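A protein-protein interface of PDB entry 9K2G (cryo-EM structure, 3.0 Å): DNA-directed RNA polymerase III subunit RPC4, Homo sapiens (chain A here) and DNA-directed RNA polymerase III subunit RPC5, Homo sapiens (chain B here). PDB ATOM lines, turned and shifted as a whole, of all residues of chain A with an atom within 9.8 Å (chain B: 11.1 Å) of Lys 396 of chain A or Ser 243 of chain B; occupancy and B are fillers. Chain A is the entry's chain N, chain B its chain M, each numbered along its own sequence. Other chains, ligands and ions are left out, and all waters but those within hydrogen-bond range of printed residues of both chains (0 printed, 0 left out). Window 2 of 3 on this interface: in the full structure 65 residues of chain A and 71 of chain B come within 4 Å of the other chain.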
ATOM      1  N   PRO A 276     -10.235  20.705 -19.042  1.00  0.00           N
ATOM      2  CA  PRO A 276      -9.516  20.677 -17.760  1.00  0.00           C
ATOM      3  C   PRO A 276     -10.267  19.917 -16.675  1.00  0.00           C
ATOM      4  O   PRO A 276     -10.642  20.498 -15.652  1.00  0.00           O
ATOM      5  CB  PRO A 276      -9.388  22.163 -17.407  1.00  0.00           C
ATOM      6  CG  PRO A 276     -10.563  22.792 -18.073  1.00  0.00           C
ATOM      7  CD  PRO A 276     -10.733  22.050 -19.368  1.00  0.00           C
ATOM      8  N   GLU A 313      -4.827   9.951 -17.158  1.00  0.00           N
ATOM      9  CA  GLU A 313      -4.677  11.279 -17.758  1.00  0.00           C
ATOM     10  C   GLU A 313      -5.102  11.278 -19.226  1.00  0.00           C
ATOM     11  O   GLU A 313      -4.496  11.943 -20.067  1.00  0.00           O
ATOM     12  CB  GLU A 313      -3.245  11.803 -17.607  1.00  0.00           C
ATOM     13  CG  GLU A 313      -2.761  11.903 -16.172  1.00  0.00           C
ATOM     14  CD  GLU A 313      -2.044  10.654 -15.707  1.00  0.00           C
ATOM     15  OE1 GLU A 313      -1.586   9.871 -16.565  1.00  0.00           O
ATOM     16  OE2 GLU A 313      -1.933  10.453 -14.479  1.00  0.00           O
ATOM     17  N   LYS A 343     -11.025  26.052 -12.695  1.00  0.00           N
ATOM     18  CA  LYS A 343      -9.805  26.706 -12.237  1.00  0.00           C
ATOM     19  C   LYS A 343      -9.120  27.480 -13.357  1.00  0.00           C
ATOM     20  O   LYS A 343      -8.509  28.524 -13.098  1.00  0.00           O
ATOM     21  CB  LYS A 343      -8.846  25.678 -11.637  1.00  0.00           C
ATOM     22  CG  LYS A 343      -9.322  25.080 -10.327  1.00  0.00           C
ATOM     23  CD  LYS A 343      -8.209  24.327  -9.626  1.00  0.00           C
ATOM     24  CE  LYS A 343      -8.650  23.823  -8.264  1.00  0.00           C
ATOM     25  NZ  LYS A 343      -9.814  22.900  -8.369  1.00  0.00           N
ATOM     26  N   VAL A 344      -9.200  26.996 -14.592  1.00  0.00           N
ATOM     27  CA  VAL A 344      -8.525  27.620 -15.715  1.00  0.00           C
ATOM     28  C   VAL A 344      -9.540  28.401 -16.538  1.00  0.00           C
ATOM     29  O   VAL A 344     -10.753  28.236 -16.413  1.00  0.00           O
ATOM     30  CB  VAL A 344      -7.789  26.587 -16.595  1.00  0.00           C
ATOM     31  CG1 VAL A 344      -6.955  25.662 -15.734  1.00  0.00           C
ATOM     32  CG2 VAL A 344      -8.781  25.800 -17.425  1.00  0.00           C
ATOM     33  N   ASP A 388      -5.520  29.435 -22.717  1.00  0.00           N
ATOM     34  CA  ASP A 388      -4.688  30.627 -22.560  1.00  0.00           C
ATOM     35  C   ASP A 388      -3.319  30.163 -22.062  1.00  0.00           C
ATOM     36  O   ASP A 388      -3.021  30.147 -20.866  1.00  0.00           O
ATOM     37  CB  ASP A 388      -5.330  31.624 -21.606  1.00  0.00           C
ATOM     38  CG  ASP A 388      -4.576  32.939 -21.539  1.00  0.00           C
ATOM     39  OD1 ASP A 388      -3.782  33.214 -22.460  1.00  0.00           O
ATOM     40  OD2 ASP A 388      -4.776  33.690 -20.563  1.00  0.00           O
ATOM     41  N   PHE A 389      -2.471  29.779 -23.023  1.00  0.00           N
ATOM     42  CA  PHE A 389      -1.192  29.166 -22.691  1.00  0.00           C
ATOM     43  C   PHE A 389      -0.276  30.113 -21.935  1.00  0.00           C
ATOM     44  O   PHE A 389       0.516  29.670 -21.098  1.00  0.00           O
ATOM     45  CB  PHE A 389      -0.504  28.668 -23.959  1.00  0.00           C
ATOM     46  CG  PHE A 389      -0.986  27.327 -24.424  1.00  0.00           C
ATOM     47  CD1 PHE A 389      -0.521  26.168 -23.825  1.00  0.00           C
ATOM     48  CD2 PHE A 389      -1.900  27.221 -25.458  1.00  0.00           C
ATOM     49  CE1 PHE A 389      -0.954  24.933 -24.250  1.00  0.00           C
ATOM     50  CE2 PHE A 389      -2.343  25.985 -25.884  1.00  0.00           C
ATOM     51  CZ  PHE A 389      -1.870  24.839 -25.278  1.00  0.00           C
ATOM     52  N   GLU A 390      -0.353  31.414 -22.221  1.00  0.00           N
ATOM     53  CA  GLU A 390       0.499  32.369 -21.516  1.00  0.00           C
ATOM     54  C   GLU A 390       0.201  32.368 -20.022  1.00  0.00           C
ATOM     55  O   GLU A 390       1.126  32.366 -19.198  1.00  0.00           O
ATOM     56  CB  GLU A 390       0.315  33.770 -22.105  1.00  0.00           C
ATOM     57  CG  GLU A 390       1.354  34.777 -21.637  1.00  0.00           C
ATOM     58  CD  GLU A 390       1.237  36.109 -22.357  1.00  0.00           C
ATOM     59  OE1 GLU A 390       0.130  36.432 -22.842  1.00  0.00           O
ATOM     60  OE2 GLU A 390       2.258  36.823 -22.452  1.00  0.00           O
ATOM     61  N   SER A 391      -1.084  32.366 -19.656  1.00  0.00           N
ATOM     62  CA  SER A 391      -1.453  32.315 -18.242  1.00  0.00           C
ATOM     63  C   SER A 391      -1.030  30.994 -17.610  1.00  0.00           C
ATOM     64  O   SER A 391      -0.536  30.979 -16.477  1.00  0.00           O
ATOM     65  CB  SER A 391      -2.961  32.524 -18.085  1.00  0.00           C
ATOM     66  OG  SER A 391      -3.687  31.473 -18.696  1.00  0.00           O
ATOM     67  N   LEU A 392      -1.217  29.881 -18.322  1.00  0.00           N
ATOM     68  CA  LEU A 392      -0.815  28.587 -17.779  1.00  0.00           C
ATOM     69  C   LEU A 392       0.692  28.507 -17.571  1.00  0.00           C
ATOM     70  O   LEU A 392       1.156  27.819 -16.657  1.00  0.00           O
ATOM     71  CB  LEU A 392      -1.281  27.458 -18.704  1.00  0.00           C
ATOM     72  CG  LEU A 392      -2.779  27.356 -18.989  1.00  0.00           C
ATOM     73  CD1 LEU A 392      -3.096  26.061 -19.727  1.00  0.00           C
ATOM     74  CD2 LEU A 392      -3.584  27.461 -17.705  1.00  0.00           C
ATOM     75  N   LEU A 393       1.467  29.205 -18.404  1.00  0.00           N
ATOM     76  CA  LEU A 393       2.919  29.171 -18.266  1.00  0.00           C
ATOM     77  C   LEU A 393       3.403  30.092 -17.154  1.00  0.00           C
ATOM     78  O   LEU A 393       4.196  29.681 -16.303  1.00  0.00           O
ATOM     79  CB  LEU A 393       3.587  29.528 -19.599  1.00  0.00           C
ATOM     80  CG  LEU A 393       3.627  28.390 -20.613  1.00  0.00           C
ATOM     81  CD1 LEU A 393       4.371  28.811 -21.869  1.00  0.00           C
ATOM     82  CD2 LEU A 393       4.271  27.156 -19.998  1.00  0.00           C
ATOM     83  N   ASP A 394       2.937  31.348 -17.143  1.00  0.00           N
ATOM     84  CA  ASP A 394       3.359  32.255 -16.077  1.00  0.00           C
ATOM     85  C   ASP A 394       2.796  31.849 -14.722  1.00  0.00           C
ATOM     86  O   ASP A 394       3.317  32.291 -13.690  1.00  0.00           O
ATOM     87  CB  ASP A 394       2.969  33.705 -16.398  1.00  0.00           C
ATOM     88  CG  ASP A 394       1.476  33.896 -16.611  1.00  0.00           C
ATOM     89  OD1 ASP A 394       0.671  33.442 -15.773  1.00  0.00           O
ATOM     90  OD2 ASP A 394       1.102  34.546 -17.612  1.00  0.00           O
ATOM     91  N   HIS A 395       1.747  31.028 -14.701  1.00  0.00           N
ATOM     92  CA  HIS A 395       1.204  30.536 -13.437  1.00  0.00           C
ATOM     93  C   HIS A 395       2.216  29.657 -12.713  1.00  0.00           C
ATOM     94  O   HIS A 395       2.452  29.823 -11.510  1.00  0.00           O
ATOM     95  CB  HIS A 395      -0.093  29.768 -13.700  1.00  0.00           C
ATOM     96  CG  HIS A 395      -0.801  29.325 -12.458  1.00  0.00           C
ATOM     97  ND1 HIS A 395      -0.510  28.140 -11.818  1.00  0.00           N
ATOM     98  CD2 HIS A 395      -1.792  29.908 -11.742  1.00  0.00           C
ATOM     99  CE1 HIS A 395      -1.289  28.011 -10.763  1.00  0.00           C
ATOM    100  NE2 HIS A 395      -2.076  29.071 -10.691  1.00  0.00           N
ATOM    101  N   LYS A 396       2.830  28.721 -13.432  1.00  0.00           N
ATOM    102  CA  LYS A 396       3.847  27.844 -12.864  1.00  0.00           C
ATOM    103  C   LYS A 396       4.918  27.510 -13.891  1.00  0.00           C
ATOM    104  O   LYS A 396       5.194  26.342 -14.165  1.00  0.00           O
ATOM    105  CB  LYS A 396       3.217  26.554 -12.331  1.00  0.00           C
ATOM    106  CG  LYS A 396       2.517  26.700 -10.985  1.00  0.00           C
ATOM    107  CD  LYS A 396       2.008  25.368 -10.472  1.00  0.00           C
ATOM    108  CE  LYS A 396       1.385  25.513  -9.093  1.00  0.00           C
ATOM    109  NZ  LYS A 396       0.910  24.209  -8.563  1.00  0.00           N
ATOM    110  N   VAL B 239     -12.048  20.422 -12.134  1.00  0.00           N
ATOM    111  CA  VAL B 239     -11.418  21.003 -10.955  1.00  0.00           C
ATOM    112  C   VAL B 239      -9.903  20.868 -10.986  1.00  0.00           C
ATOM    113  O   VAL B 239      -9.242  21.124  -9.978  1.00  0.00           O
ATOM    114  CB  VAL B 239     -11.992  20.388  -9.660  1.00  0.00           C
ATOM    115  CG1 VAL B 239     -13.441  20.792  -9.472  1.00  0.00           C
ATOM    116  CG2 VAL B 239     -11.854  18.872  -9.684  1.00  0.00           C
ATOM    117  N   LYS B 240      -9.335  20.467 -12.117  1.00  0.00           N
ATOM    118  CA  LYS B 240      -7.894  20.299 -12.208  1.00  0.00           C
ATOM    119  C   LYS B 240      -7.188  21.651 -12.260  1.00  0.00           C
ATOM    120  O   LYS B 240      -7.684  22.608 -12.865  1.00  0.00           O
ATOM    121  CB  LYS B 240      -7.523  19.462 -13.429  1.00  0.00           C
ATOM    122  CG  LYS B 240      -7.892  18.000 -13.285  1.00  0.00           C
ATOM    123  CD  LYS B 240      -6.858  17.092 -13.933  1.00  0.00           C
ATOM    124  CE  LYS B 240      -7.011  15.658 -13.454  1.00  0.00           C
ATOM    125  NZ  LYS B 240      -6.005  14.750 -14.069  1.00  0.00           N
ATOM    126  N   SER B 241      -6.028  21.724 -11.615  1.00  0.00           N
ATOM    127  CA  SER B 241      -5.266  22.956 -11.549  1.00  0.00           C
ATOM    128  C   SER B 241      -4.679  23.295 -12.917  1.00  0.00           C
ATOM    129  O   SER B 241      -4.559  22.425 -13.783  1.00  0.00           O
ATOM    130  CB  SER B 241      -4.152  22.831 -10.513  1.00  0.00           C
ATOM    131  OG  SER B 241      -3.139  21.947 -10.958  1.00  0.00           O
ATOM    132  N   PRO B 242      -4.323  24.567 -13.144  1.00  0.00           N
ATOM    133  CA  PRO B 242      -3.682  24.929 -14.419  1.00  0.00           C
ATOM    134  C   PRO B 242      -2.430  24.128 -14.721  1.00  0.00           C
ATOM    135  O   PRO B 242      -2.198  23.761 -15.882  1.00  0.00           O
ATOM    136  CB  PRO B 242      -3.377  26.419 -14.233  1.00  0.00           C
ATOM    137  CG  PRO B 242      -4.412  26.891 -13.275  1.00  0.00           C
ATOM    138  CD  PRO B 242      -4.636  25.753 -12.324  1.00  0.00           C
ATOM    139  N   SER B 243      -1.613  23.837 -13.708  1.00  0.00           N
ATOM    140  CA  SER B 243      -0.448  22.980 -13.920  1.00  0.00           C
ATOM    141  C   SER B 243      -0.866  21.578 -14.348  1.00  0.00           C
ATOM    142  O   SER B 243      -0.274  21.001 -15.268  1.00  0.00           O
ATOM    143  CB  SER B 243       0.400  22.926 -12.652  1.00  0.00           C
ATOM    144  OG  SER B 243       1.423  21.947 -12.762  1.00  0.00           O
ATOM    145  N   GLU B 244      -1.887  21.023 -13.690  1.00  0.00           N
ATOM    146  CA  GLU B 244      -2.374  19.700 -14.063  1.00  0.00           C
ATOM    147  C   GLU B 244      -2.935  19.692 -15.477  1.00  0.00           C
ATOM    148  O   GLU B 244      -2.707  18.746 -16.238  1.00  0.00           O
ATOM    149  CB  GLU B 244      -3.422  19.230 -13.055  1.00  0.00           C
ATOM    150  CG  GLU B 244      -2.851  18.857 -11.694  1.00  0.00           C
ATOM    151  CD  GLU B 244      -3.900  18.852 -10.597  1.00  0.00           C
ATOM    152  OE1 GLU B 244      -4.934  19.539 -10.759  1.00  0.00           O
ATOM    153  OE2 GLU B 244      -3.691  18.162  -9.578  1.00  0.00           O
ATOM    154  N   TYR B 245      -3.676  20.742 -15.847  1.00  0.00           N
ATOM    155  CA  TYR B 245      -4.207  20.827 -17.205  1.00  0.00           C
ATOM    156  C   TYR B 245      -3.088  20.917 -18.233  1.00  0.00           C
ATOM    157  O   TYR B 245      -3.137  20.257 -19.282  1.00  0.00           O
ATOM    158  CB  TYR B 245      -5.138  22.034 -17.322  1.00  0.00           C
ATOM    159  CG  TYR B 245      -5.958  22.058 -18.594  1.00  0.00           C
ATOM    160  CD1 TYR B 245      -6.254  20.880 -19.267  1.00  0.00           C
ATOM    161  CD2 TYR B 245      -6.423  23.253 -19.121  1.00  0.00           C
ATOM    162  CE1 TYR B 245      -6.999  20.892 -20.430  1.00  0.00           C
ATOM    163  CE2 TYR B 245      -7.169  23.277 -20.282  1.00  0.00           C
ATOM    164  CZ  TYR B 245      -7.451  22.093 -20.936  1.00  0.00           C
ATOM    165  OH  TYR B 245      -8.194  22.118 -22.093  1.00  0.00           O
ATOM    166  N   LEU B 246      -2.066  21.730 -17.951  1.00  0.00           N
ATOM    167  CA  LEU B 246      -0.932  21.850 -18.866  1.00  0.00           C
ATOM    168  C   LEU B 246      -0.201  20.525 -19.015  1.00  0.00           C
ATOM    169  O   LEU B 246       0.210  20.154 -20.120  1.00  0.00           O
ATOM    170  CB  LEU B 246       0.019  22.937 -18.369  1.00  0.00           C
ATOM    171  CG  LEU B 246       1.385  23.043 -19.051  1.00  0.00           C
ATOM    172  CD1 LEU B 246       1.246  23.354 -20.536  1.00  0.00           C
ATOM    173  CD2 LEU B 246       2.244  24.091 -18.352  1.00  0.00           C
ATOM    174  N   MET B 247      -0.027  19.795 -17.911  1.00  0.00           N
ATOM    175  CA  MET B 247       0.577  18.467 -17.992  1.00  0.00           C
ATOM    176  C   MET B 247      -0.293  17.515 -18.805  1.00  0.00           C
ATOM    177  O   MET B 247       0.225  16.692 -19.568  1.00  0.00           O
ATOM    178  CB  MET B 247       0.809  17.913 -16.587  1.00  0.00           C
ATOM    179  CG  MET B 247       1.837  18.677 -15.759  1.00  0.00           C
ATOM    180  SD  MET B 247       3.497  18.673 -16.469  1.00  0.00           S
ATOM    181  CE  MET B 247       3.571  20.312 -17.191  1.00  0.00           C
ATOM    182  N   MET B 248      -1.611  17.606 -18.649  1.00  0.00           N
ATOM    183  CA  MET B 248      -2.514  16.702 -19.355  1.00  0.00           C
ATOM    184  C   MET B 248      -2.469  16.931 -20.860  1.00  0.00           C
ATOM    185  O   MET B 248      -2.332  15.980 -21.641  1.00  0.00           O
ATOM    186  CB  MET B 248      -3.938  16.864 -18.821  1.00  0.00           C
ATOM    187  CG  MET B 248      -4.969  16.037 -19.578  1.00  0.00           C
ATOM    188  SD  MET B 248      -6.646  16.258 -18.957  1.00  0.00           S
ATOM    189  CE  MET B 248      -6.480  15.631 -17.287  1.00  0.00           C
ATOM    190  N   LEU B 249      -2.576  18.188 -21.293  1.00  0.00           N
ATOM    191  CA  LEU B 249      -2.633  18.457 -22.727  1.00  0.00           C
ATOM    192  C   LEU B 249      -1.264  18.460 -23.394  1.00  0.00           C
ATOM    193  O   LEU B 249      -1.194  18.542 -24.625  1.00  0.00           O
ATOM    194  CB  LEU B 249      -3.358  19.786 -22.988  1.00  0.00           C
ATOM    195  CG  LEU B 249      -2.844  21.083 -22.365  1.00  0.00           C
ATOM    196  CD1 LEU B 249      -1.839  21.762 -23.277  1.00  0.00           C
ATOM    197  CD2 LEU B 249      -4.007  22.016 -22.061  1.00  0.00           C
ATOM    198  N   MET B 250      -0.182  18.367 -22.622  1.00  0.00           N
ATOM    199  CA  MET B 250       1.169  18.210 -23.154  1.00  0.00           C
ATOM    200  C   MET B 250       1.857  17.063 -22.418  1.00  0.00           C
ATOM    201  O   MET B 250       2.739  17.287 -21.577  1.00  0.00           O
ATOM    202  CB  MET B 250       1.976  19.506 -23.028  1.00  0.00           C
ATOM    203  CG  MET B 250       1.474  20.642 -23.901  1.00  0.00           C
ATOM    204  SD  MET B 250       1.499  20.255 -25.662  1.00  0.00           S
ATOM    205  CE  MET B 250       3.262  20.113 -25.950  1.00  0.00           C
ATOM    206  N   PRO B 251       1.471  15.818 -22.708  1.00  0.00           N
ATOM    207  CA  PRO B 251       2.063  14.691 -21.997  1.00  0.00           C
ATOM    208  C   PRO B 251       3.528  14.538 -22.335  1.00  0.00           C
ATOM    209  O   PRO B 251       3.959  14.859 -23.463  1.00  0.00           O
ATOM    210  CB  PRO B 251       1.240  13.487 -22.495  1.00  0.00           C
ATOM    211  CG  PRO B 251       0.764  13.904 -23.839  1.00  0.00           C
ATOM    212  CD  PRO B 251       0.518  15.386 -23.746  1.00  0.00           C
ATOM    213  N   PRO B 252       4.346  14.057 -21.401  1.00  0.00           N
ATOM    214  CA  PRO B 252       5.761  13.831 -21.699  1.00  0.00           C
ATOM    215  C   PRO B 252       5.950  12.727 -22.726  1.00  0.00           C
ATOM    216  O   PRO B 252       5.119  11.826 -22.867  1.00  0.00           O
ATOM    217  CB  PRO B 252       6.358  13.435 -20.344  1.00  0.00           C
ATOM    218  CG  PRO B 252       5.383  13.952 -19.330  1.00  0.00           C
ATOM    219  CD  PRO B 252       4.039  13.833 -19.981  1.00  0.00           C
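NZ of Lys 343 of chain A sits at hydrogen-bond distance from O of Val 239 of chain B, 2.5 Å away.
The side-chain carboxylate of Glu 244 of chain B lies within hydrogen-bond range of the backbone NH of Ser 241 of chain B, 2.6 Å away.
Among the printed residues, merely in contact across the chains: Phe 389 of chain A with Leu 249 of chain B (3.4 Å), Lys 343 of chain A with Lys 240 of chain B (3.5 Å), Pro 276 of chain A with Tyr 245 of chain B (3.5 Å), Val 344 of chain A with Pro 242 of chain B (3.6 Å), Leu 392 of chain A with Pro 242 of chain B (3.6 Å), Lys 396 of chain A with Ser 243 of chain B (3.6 Å), Pro 276 of chain A with Lys 240 of chain B (3.8 Å), Lys 343 of chain A with Ser 241 of chain B (3.8 Å), Pro 276 of chain A with Val 239 of chain B (3.8 Å) and Val 344 of chain A with Tyr 245 of chain B (3.9 Å).
Printed residues of chain A within 4 Å of Ser 243 of chain B: Lys 396.
Ser 241 of chain B touches one residue of chain A.
Printed residues of chain A within 4 Å of Pro 242 of chain B: Val 344 and Leu 392.
Printed residues of chain B within 4 Å of Lys 343 of chain A: Val 239 (2.5 Å), Lys 240 (3.5 Å) and Ser 241 (3.8 Å).
Printed residues of chain B within 4 Å of Val 344 of chain A: Pro 242 (3.6 Å) and Tyr 245 (3.9 Å).
Of the printed residues of chain B, Pro 276 of chain A touches Val 239, Lys 240 and Tyr 245.
Printed residues of chain A within 4 Å of Tyr 245 of chain B: Pro 276 and Val 344.
Of the printed residues of chain A, Lys 240 of chain B touches Pro 276 and Lys 343.
Glu 390 of chain A touches none of the printed residues of chain B.
Of the 14 printed residues of chain B, 7 touch a printed residue of chain A.
Of the 13 printed residues of chain A, 6 touch a printed residue of chain B.
Printed residues of chain A that touch a printed residue of chain B: Pro 276, Lys 343, Val 344, Phe 389, Leu 392 and Lys 396.
Among the printed residues, 11 pairs touch across the chains.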
